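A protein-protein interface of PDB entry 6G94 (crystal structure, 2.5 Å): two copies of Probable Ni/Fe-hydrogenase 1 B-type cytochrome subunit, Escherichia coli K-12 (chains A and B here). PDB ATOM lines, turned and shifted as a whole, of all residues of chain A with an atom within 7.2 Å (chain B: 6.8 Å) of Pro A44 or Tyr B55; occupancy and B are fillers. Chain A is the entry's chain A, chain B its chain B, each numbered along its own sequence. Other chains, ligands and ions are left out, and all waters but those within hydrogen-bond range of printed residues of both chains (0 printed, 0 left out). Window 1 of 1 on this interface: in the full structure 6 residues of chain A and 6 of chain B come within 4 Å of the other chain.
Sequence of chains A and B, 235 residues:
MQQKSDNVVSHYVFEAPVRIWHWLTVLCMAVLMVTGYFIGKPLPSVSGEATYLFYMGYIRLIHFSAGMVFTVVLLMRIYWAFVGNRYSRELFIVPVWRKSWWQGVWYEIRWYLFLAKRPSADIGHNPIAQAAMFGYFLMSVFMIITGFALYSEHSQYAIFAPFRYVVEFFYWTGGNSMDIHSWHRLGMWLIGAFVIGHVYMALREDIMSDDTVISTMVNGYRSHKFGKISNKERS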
ATOM      1  N   PHE A  38     -18.537  -8.579   5.249  1.00  0.00           N
ATOM      2  CA  PHE A  38     -17.921  -7.860   6.352  1.00  0.00           C
ATOM      3  C   PHE A  38     -17.810  -6.338   6.159  1.00  0.00           C
ATOM      4  O   PHE A  38     -17.467  -5.620   7.098  1.00  0.00           O
ATOM      5  CB  PHE A  38     -16.560  -8.471   6.658  1.00  0.00           C
ATOM      6  CG  PHE A  38     -16.646  -9.834   7.243  1.00  0.00           C
ATOM      7  CD1 PHE A  38     -17.461 -10.081   8.331  1.00  0.00           C
ATOM      8  CD2 PHE A  38     -15.913 -10.884   6.702  1.00  0.00           C
ATOM      9  CE1 PHE A  38     -17.551 -11.356   8.870  1.00  0.00           C
ATOM     10  CE2 PHE A  38     -15.992 -12.165   7.234  1.00  0.00           C
ATOM     11  CZ  PHE A  38     -16.823 -12.402   8.320  1.00  0.00           C
ATOM     12  N   LYS A  41     -21.562  -6.155   7.765  1.00  0.00           N
ATOM     13  CA  LYS A  41     -21.499  -6.626   9.145  1.00  0.00           C
ATOM     14  C   LYS A  41     -20.029  -6.833   9.511  1.00  0.00           C
ATOM     15  O   LYS A  41     -19.509  -7.964   9.417  1.00  0.00           O
ATOM     16  CB  LYS A  41     -22.312  -7.911   9.328  1.00  0.00           C
ATOM     17  CG  LYS A  41     -23.813  -7.723   9.189  1.00  0.00           C
ATOM     18  CD  LYS A  41     -24.437  -7.209  10.487  1.00  0.00           C
ATOM     19  CE  LYS A  41     -25.925  -6.884  10.318  1.00  0.00           C
ATOM     20  NZ  LYS A  41     -26.503  -6.157  11.491  1.00  0.00           N
ATOM     21  N   PRO A  42     -19.339  -5.739   9.897  1.00  0.00           N
ATOM     22  CA  PRO A  42     -17.879  -5.767  10.120  1.00  0.00           C
ATOM     23  C   PRO A  42     -17.466  -6.687  11.244  1.00  0.00           C
ATOM     24  O   PRO A  42     -18.267  -6.977  12.140  1.00  0.00           O
ATOM     25  CB  PRO A  42     -17.553  -4.331  10.496  1.00  0.00           C
ATOM     26  CG  PRO A  42     -18.651  -3.532   9.867  1.00  0.00           C
ATOM     27  CD  PRO A  42     -19.878  -4.374  10.035  1.00  0.00           C
ATOM     28  N   LEU A  43     -16.215  -7.125  11.197  1.00  0.00           N
ATOM     29  CA  LEU A  43     -15.667  -8.038  12.184  1.00  0.00           C
ATOM     30  C   LEU A  43     -15.652  -7.344  13.525  1.00  0.00           C
ATOM     31  O   LEU A  43     -15.912  -6.143  13.574  1.00  0.00           O
ATOM     32  CB  LEU A  43     -14.258  -8.449  11.773  1.00  0.00           C
ATOM     33  CG  LEU A  43     -14.193  -9.417  10.586  1.00  0.00           C
ATOM     34  CD1 LEU A  43     -12.971  -9.191   9.704  1.00  0.00           C
ATOM     35  CD2 LEU A  43     -14.279 -10.851  11.068  1.00  0.00           C
ATOM     36  N   PRO A  44     -15.346  -8.074  14.619  1.00  0.00           N
ATOM     37  CA  PRO A  44     -15.194  -7.376  15.902  1.00  0.00           C
ATOM     38  C   PRO A  44     -14.161  -6.232  15.848  1.00  0.00           C
ATOM     39  O   PRO A  44     -13.315  -6.207  14.946  1.00  0.00           O
ATOM     40  CB  PRO A  44     -14.727  -8.486  16.839  1.00  0.00           C
ATOM     41  CG  PRO A  44     -15.368  -9.698  16.283  1.00  0.00           C
ATOM     42  CD  PRO A  44     -15.233  -9.535  14.796  1.00  0.00           C
ATOM     43  N   SER A  45     -14.229  -5.297  16.794  1.00  0.00           N
ATOM     44  CA  SER A  45     -13.359  -4.140  16.752  1.00  0.00           C
ATOM     45  C   SER A  45     -11.987  -4.489  17.287  1.00  0.00           C
ATOM     46  O   SER A  45     -11.835  -5.269  18.234  1.00  0.00           O
ATOM     47  CB  SER A  45     -13.954  -3.008  17.581  1.00  0.00           C
ATOM     48  OG  SER A  45     -13.308  -1.775  17.342  1.00  0.00           O
ATOM     49  N   VAL A  46     -10.986  -3.889  16.663  1.00  0.00           N
ATOM     50  CA  VAL A  46      -9.625  -3.891  17.189  1.00  0.00           C
ATOM     51  C   VAL A  46      -9.307  -2.569  17.889  1.00  0.00           C
ATOM     52  O   VAL A  46     -10.120  -1.632  17.890  1.00  0.00           O
ATOM     53  CB  VAL A  46      -8.606  -4.088  16.068  1.00  0.00           C
ATOM     54  CG1 VAL A  46      -8.697  -5.514  15.549  1.00  0.00           C
ATOM     55  CG2 VAL A  46      -8.813  -3.063  14.945  1.00  0.00           C
ATOM     56  N   LEU B  43      -5.804 -14.253  15.201  1.00  0.00           N
ATOM     57  CA  LEU B  43      -6.288 -13.046  14.572  1.00  0.00           C
ATOM     58  C   LEU B  43      -5.946 -11.817  15.459  1.00  0.00           C
ATOM     59  O   LEU B  43      -5.429 -11.975  16.568  1.00  0.00           O
ATOM     60  CB  LEU B  43      -7.791 -13.203  14.322  1.00  0.00           C
ATOM     61  CG  LEU B  43      -8.207 -14.206  13.238  1.00  0.00           C
ATOM     62  CD1 LEU B  43      -9.526 -14.851  13.609  1.00  0.00           C
ATOM     63  CD2 LEU B  43      -8.303 -13.556  11.862  1.00  0.00           C
ATOM     64  N   SER B  45      -6.448  -8.887  18.250  1.00  0.00           N
ATOM     65  CA  SER B  45      -7.129  -8.984  19.551  1.00  0.00           C
ATOM     66  C   SER B  45      -8.428  -8.226  19.539  1.00  0.00           C
ATOM     67  O   SER B  45      -8.569  -7.251  18.812  1.00  0.00           O
ATOM     68  CB  SER B  45      -6.255  -8.471  20.699  1.00  0.00           C
ATOM     69  OG  SER B  45      -6.821  -8.810  21.955  1.00  0.00           O
ATOM     70  N   VAL B  46      -9.376  -8.724  20.327  1.00  0.00           N
ATOM     71  CA  VAL B  46     -10.652  -8.056  20.591  1.00  0.00           C
ATOM     72  C   VAL B  46     -10.631  -7.604  22.034  1.00  0.00           C
ATOM     73  O   VAL B  46      -9.702  -7.923  22.789  1.00  0.00           O
ATOM     74  CB  VAL B  46     -11.891  -8.965  20.366  1.00  0.00           C
ATOM     75  CG1 VAL B  46     -12.103  -9.230  18.894  1.00  0.00           C
ATOM     76  CG2 VAL B  46     -11.777 -10.268  21.143  1.00  0.00           C
ATOM     77  N   SER B  47     -11.665  -6.874  22.424  1.00  0.00           N
ATOM     78  CA  SER B  47     -11.746  -6.386  23.790  1.00  0.00           C
ATOM     79  C   SER B  47     -13.186  -6.283  24.165  1.00  0.00           C
ATOM     80  O   SER B  47     -14.016  -5.857  23.365  1.00  0.00           O
ATOM     81  CB  SER B  47     -11.056  -5.024  23.950  1.00  0.00           C
ATOM     82  OG  SER B  47     -11.703  -4.032  23.177  1.00  0.00           O
ATOM     83  N   TYR B  52     -18.851 -13.085  27.702  1.00  0.00           N
ATOM     84  CA  TYR B  52     -19.693 -13.152  26.513  1.00  0.00           C
ATOM     85  C   TYR B  52     -18.882 -13.307  25.235  1.00  0.00           C
ATOM     86  O   TYR B  52     -19.427 -13.185  24.140  1.00  0.00           O
ATOM     87  CB  TYR B  52     -20.605 -11.917  26.426  1.00  0.00           C
ATOM     88  CG  TYR B  52     -21.492 -11.752  27.627  1.00  0.00           C
ATOM     89  CD1 TYR B  52     -22.394 -12.741  27.971  1.00  0.00           C
ATOM     90  CD2 TYR B  52     -21.425 -10.611  28.424  1.00  0.00           C
ATOM     91  CE1 TYR B  52     -23.209 -12.606  29.075  1.00  0.00           C
ATOM     92  CE2 TYR B  52     -22.241 -10.462  29.536  1.00  0.00           C
ATOM     93  CZ  TYR B  52     -23.131 -11.471  29.855  1.00  0.00           C
ATOM     94  OH  TYR B  52     -23.954 -11.371  30.947  1.00  0.00           O
ATOM     95  N   LEU B  53     -17.587 -13.576  25.371  1.00  0.00           N
ATOM     96  CA  LEU B  53     -16.716 -13.659  24.213  1.00  0.00           C
ATOM     97  C   LEU B  53     -16.033 -14.994  24.214  1.00  0.00           C
ATOM     98  O   LEU B  53     -15.619 -15.464  25.265  1.00  0.00           O
ATOM     99  CB  LEU B  53     -15.697 -12.518  24.216  1.00  0.00           C
ATOM    100  CG  LEU B  53     -16.232 -11.091  24.058  1.00  0.00           C
ATOM    101  CD1 LEU B  53     -15.093 -10.095  24.085  1.00  0.00           C
ATOM    102  CD2 LEU B  53     -17.062 -10.918  22.792  1.00  0.00           C
ATOM    103  N   PHE B  54     -15.929 -15.609  23.032  1.00  0.00           N
ATOM    104  CA  PHE B  54     -15.397 -16.963  22.907  1.00  0.00           C
ATOM    105  C   PHE B  54     -14.817 -17.234  21.517  1.00  0.00           C
ATOM    106  O   PHE B  54     -14.821 -18.383  21.050  1.00  0.00           O
ATOM    107  CB  PHE B  54     -16.500 -17.978  23.236  1.00  0.00           C
ATOM    108  CG  PHE B  54     -15.995 -19.351  23.594  1.00  0.00           C
ATOM    109  CD1 PHE B  54     -15.252 -19.561  24.754  1.00  0.00           C
ATOM    110  CD2 PHE B  54     -16.288 -20.444  22.786  1.00  0.00           C
ATOM    111  CE1 PHE B  54     -14.804 -20.834  25.094  1.00  0.00           C
ATOM    112  CE2 PHE B  54     -15.845 -21.719  23.124  1.00  0.00           C
ATOM    113  CZ  PHE B  54     -15.105 -21.916  24.281  1.00  0.00           C
ATOM    114  N   TYR B  55     -14.323 -16.184  20.861  1.00  0.00           N
ATOM    115  CA  TYR B  55     -13.833 -16.291  19.482  1.00  0.00           C
ATOM    116  C   TYR B  55     -12.752 -17.358  19.269  1.00  0.00           C
ATOM    117  O   TYR B  55     -12.888 -18.237  18.408  1.00  0.00           O
ATOM    118  CB  TYR B  55     -13.329 -14.942  19.010  1.00  0.00           C
ATOM    119  CG  TYR B  55     -14.432 -13.933  18.848  1.00  0.00           C
ATOM    120  CD1 TYR B  55     -15.460 -14.130  17.921  1.00  0.00           C
ATOM    121  CD2 TYR B  55     -14.457 -12.770  19.620  1.00  0.00           C
ATOM    122  CE1 TYR B  55     -16.472 -13.189  17.761  1.00  0.00           C
ATOM    123  CE2 TYR B  55     -15.460 -11.825  19.464  1.00  0.00           C
ATOM    124  CZ  TYR B  55     -16.464 -12.038  18.536  1.00  0.00           C
ATOM    125  OH  TYR B  55     -17.451 -11.087  18.390  1.00  0.00           O
ATOM    126  N   MET B  56     -11.684 -17.294  20.056  1.00  0.00           N
ATOM    127  CA  MET B  56     -10.635 -18.314  19.970  1.00  0.00           C
ATOM    128  C   MET B  56     -11.195 -19.684  20.356  1.00  0.00           C
ATOM    129  O   MET B  56     -10.917 -20.681  19.706  1.00  0.00           O
ATOM    130  CB  MET B  56      -9.441 -17.955  20.857  1.00  0.00           C
ATOM    131  CG  MET B  56      -8.438 -19.089  21.077  1.00  0.00           C
ATOM    132  SD  MET B  56      -7.411 -19.556  19.654  1.00  0.00           S
ATOM    133  CE  MET B  56      -6.799 -17.974  19.056  1.00  0.00           C
ATOM    134  N   GLY B  57     -12.013 -19.723  21.397  1.00  0.00           N
ATOM    135  CA  GLY B  57     -12.618 -20.960  21.825  1.00  0.00           C
ATOM    136  C   GLY B  57     -13.453 -21.606  20.740  1.00  0.00           C
ATOM    137  O   GLY B  57     -13.453 -22.820  20.643  1.00  0.00           O
ATOM    138  N   TYR B  58     -14.139 -20.821  19.911  1.00  0.00           N
ATOM    139  CA  TYR B  58     -14.946 -21.368  18.806  1.00  0.00           C
ATOM    140  C   TYR B  58     -14.083 -21.916  17.677  1.00  0.00           C
ATOM    141  O   TYR B  58     -14.375 -22.966  17.103  1.00  0.00           O
ATOM    142  CB  TYR B  58     -15.907 -20.339  18.212  1.00  0.00           C
ATOM    143  CG  TYR B  58     -17.192 -20.169  18.976  1.00  0.00           C
ATOM    144  CD1 TYR B  58     -17.933 -21.275  19.426  1.00  0.00           C
ATOM    145  CD2 TYR B  58     -17.687 -18.891  19.245  1.00  0.00           C
ATOM    146  CE1 TYR B  58     -19.115 -21.099  20.136  1.00  0.00           C
ATOM    147  CE2 TYR B  58     -18.857 -18.707  19.953  1.00  0.00           C
ATOM    148  CZ  TYR B  58     -19.559 -19.806  20.403  1.00  0.00           C
ATOM    149  OH  TYR B  58     -20.712 -19.597  21.103  1.00  0.00           O
ATOM    150  N   ILE B  59     -13.024 -21.182  17.366  1.00  0.00           N
ATOM    151  CA  ILE B  59     -12.032 -21.587  16.398  1.00  0.00           C
ATOM    152  C   ILE B  59     -11.468 -22.943  16.789  1.00  0.00           C
ATOM    153  O   ILE B  59     -11.415 -23.841  15.968  1.00  0.00           O
ATOM    154  CB  ILE B  59     -10.933 -20.507  16.295  1.00  0.00           C
ATOM    155  CG1 ILE B  59     -11.445 -19.345  15.465  1.00  0.00           C
ATOM    156  CG2 ILE B  59      -9.618 -21.041  15.724  1.00  0.00           C
ATOM    157  CD1 ILE B  59     -10.585 -18.119  15.566  1.00  0.00           C
ATOM    158  N   ARG B  60     -11.062 -23.071  18.047  1.00  0.00           N
ATOM    159  CA  ARG B  60     -10.516 -24.306  18.578  1.00  0.00           C
ATOM    160  C   ARG B  60     -11.537 -25.440  18.592  1.00  0.00           C
ATOM    161  O   ARG B  60     -11.195 -26.608  18.475  1.00  0.00           O
ATOM    162  CB  ARG B  60      -9.997 -24.082  19.988  1.00  0.00           C
ATOM    163  CG  ARG B  60      -8.775 -23.216  20.040  1.00  0.00           C
ATOM    164  CD  ARG B  60      -8.340 -22.923  21.442  1.00  0.00           C
ATOM    165  NE  ARG B  60      -7.925 -24.122  22.111  1.00  0.00           N
ATOM    166  CZ  ARG B  60      -8.486 -24.561  23.219  1.00  0.00           C
ATOM    167  NH1 ARG B  60      -8.077 -25.674  23.783  1.00  0.00           N
ATOM    168  NH2 ARG B  60      -9.465 -23.891  23.763  1.00  0.00           N
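Pro A44 touches just these residues of chain B: Val B46 (3.4 Å) and Tyr B55 (3.3 Å).
Printed residues of chain A within 4 Å of Val B46: Pro A44 and Ser A45.
Of the printed residues of chain B, Ser A45 touches Ser B45 (3.9 Å) and Val B46 (3.8 Å).
Of the printed residues of chain B, Val A46 touches Ser B45 (3.7 Å).
Of the printed residues of chain A, Ser B45 touches Ser A45 and Val A46.
Phe A38 touches none of the printed residues of chain B.
Leu B43 touches none of the printed residues of chain A.
The nearest printed residue of chain A that does not touch Ser B45 is Pro A44 (6.2 Å).
Of the 7 printed residues of chain A, 3 touch a printed residue of chain B.
Printed residues of chain A that touch a printed residue of chain B: Pro A44, Ser A45 and Val A46.
Hydrophobic or aromatic side chains of chain A that line the printed part of chain B: Pro A44 and Val A46.
Printed residues of chain B that touch a printed residue of chain A: Ser B45, Val B46 and Tyr B55.
Hydrophobic or aromatic side chains of chain B within 4 Å of the printed part of chain A: Val B46 and Tyr B55.
Ser B45 touches its own counterpart, Ser A45.
Ser A45 touches Val B46, and with the chains exchanged Val A46 touches Ser B45.
Pro A44 touches Val B46 (CB to CG1, 3.4 Å).
Pro A44 touches Tyr B55.
O of Ser A45 touches O of Ser B45, at 3.9 Å.
Val B46 touches Ser A45 (CA to O, 3.8 Å).
CG1 of Val A46 touches O of Ser B45, at 3.7 Å.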
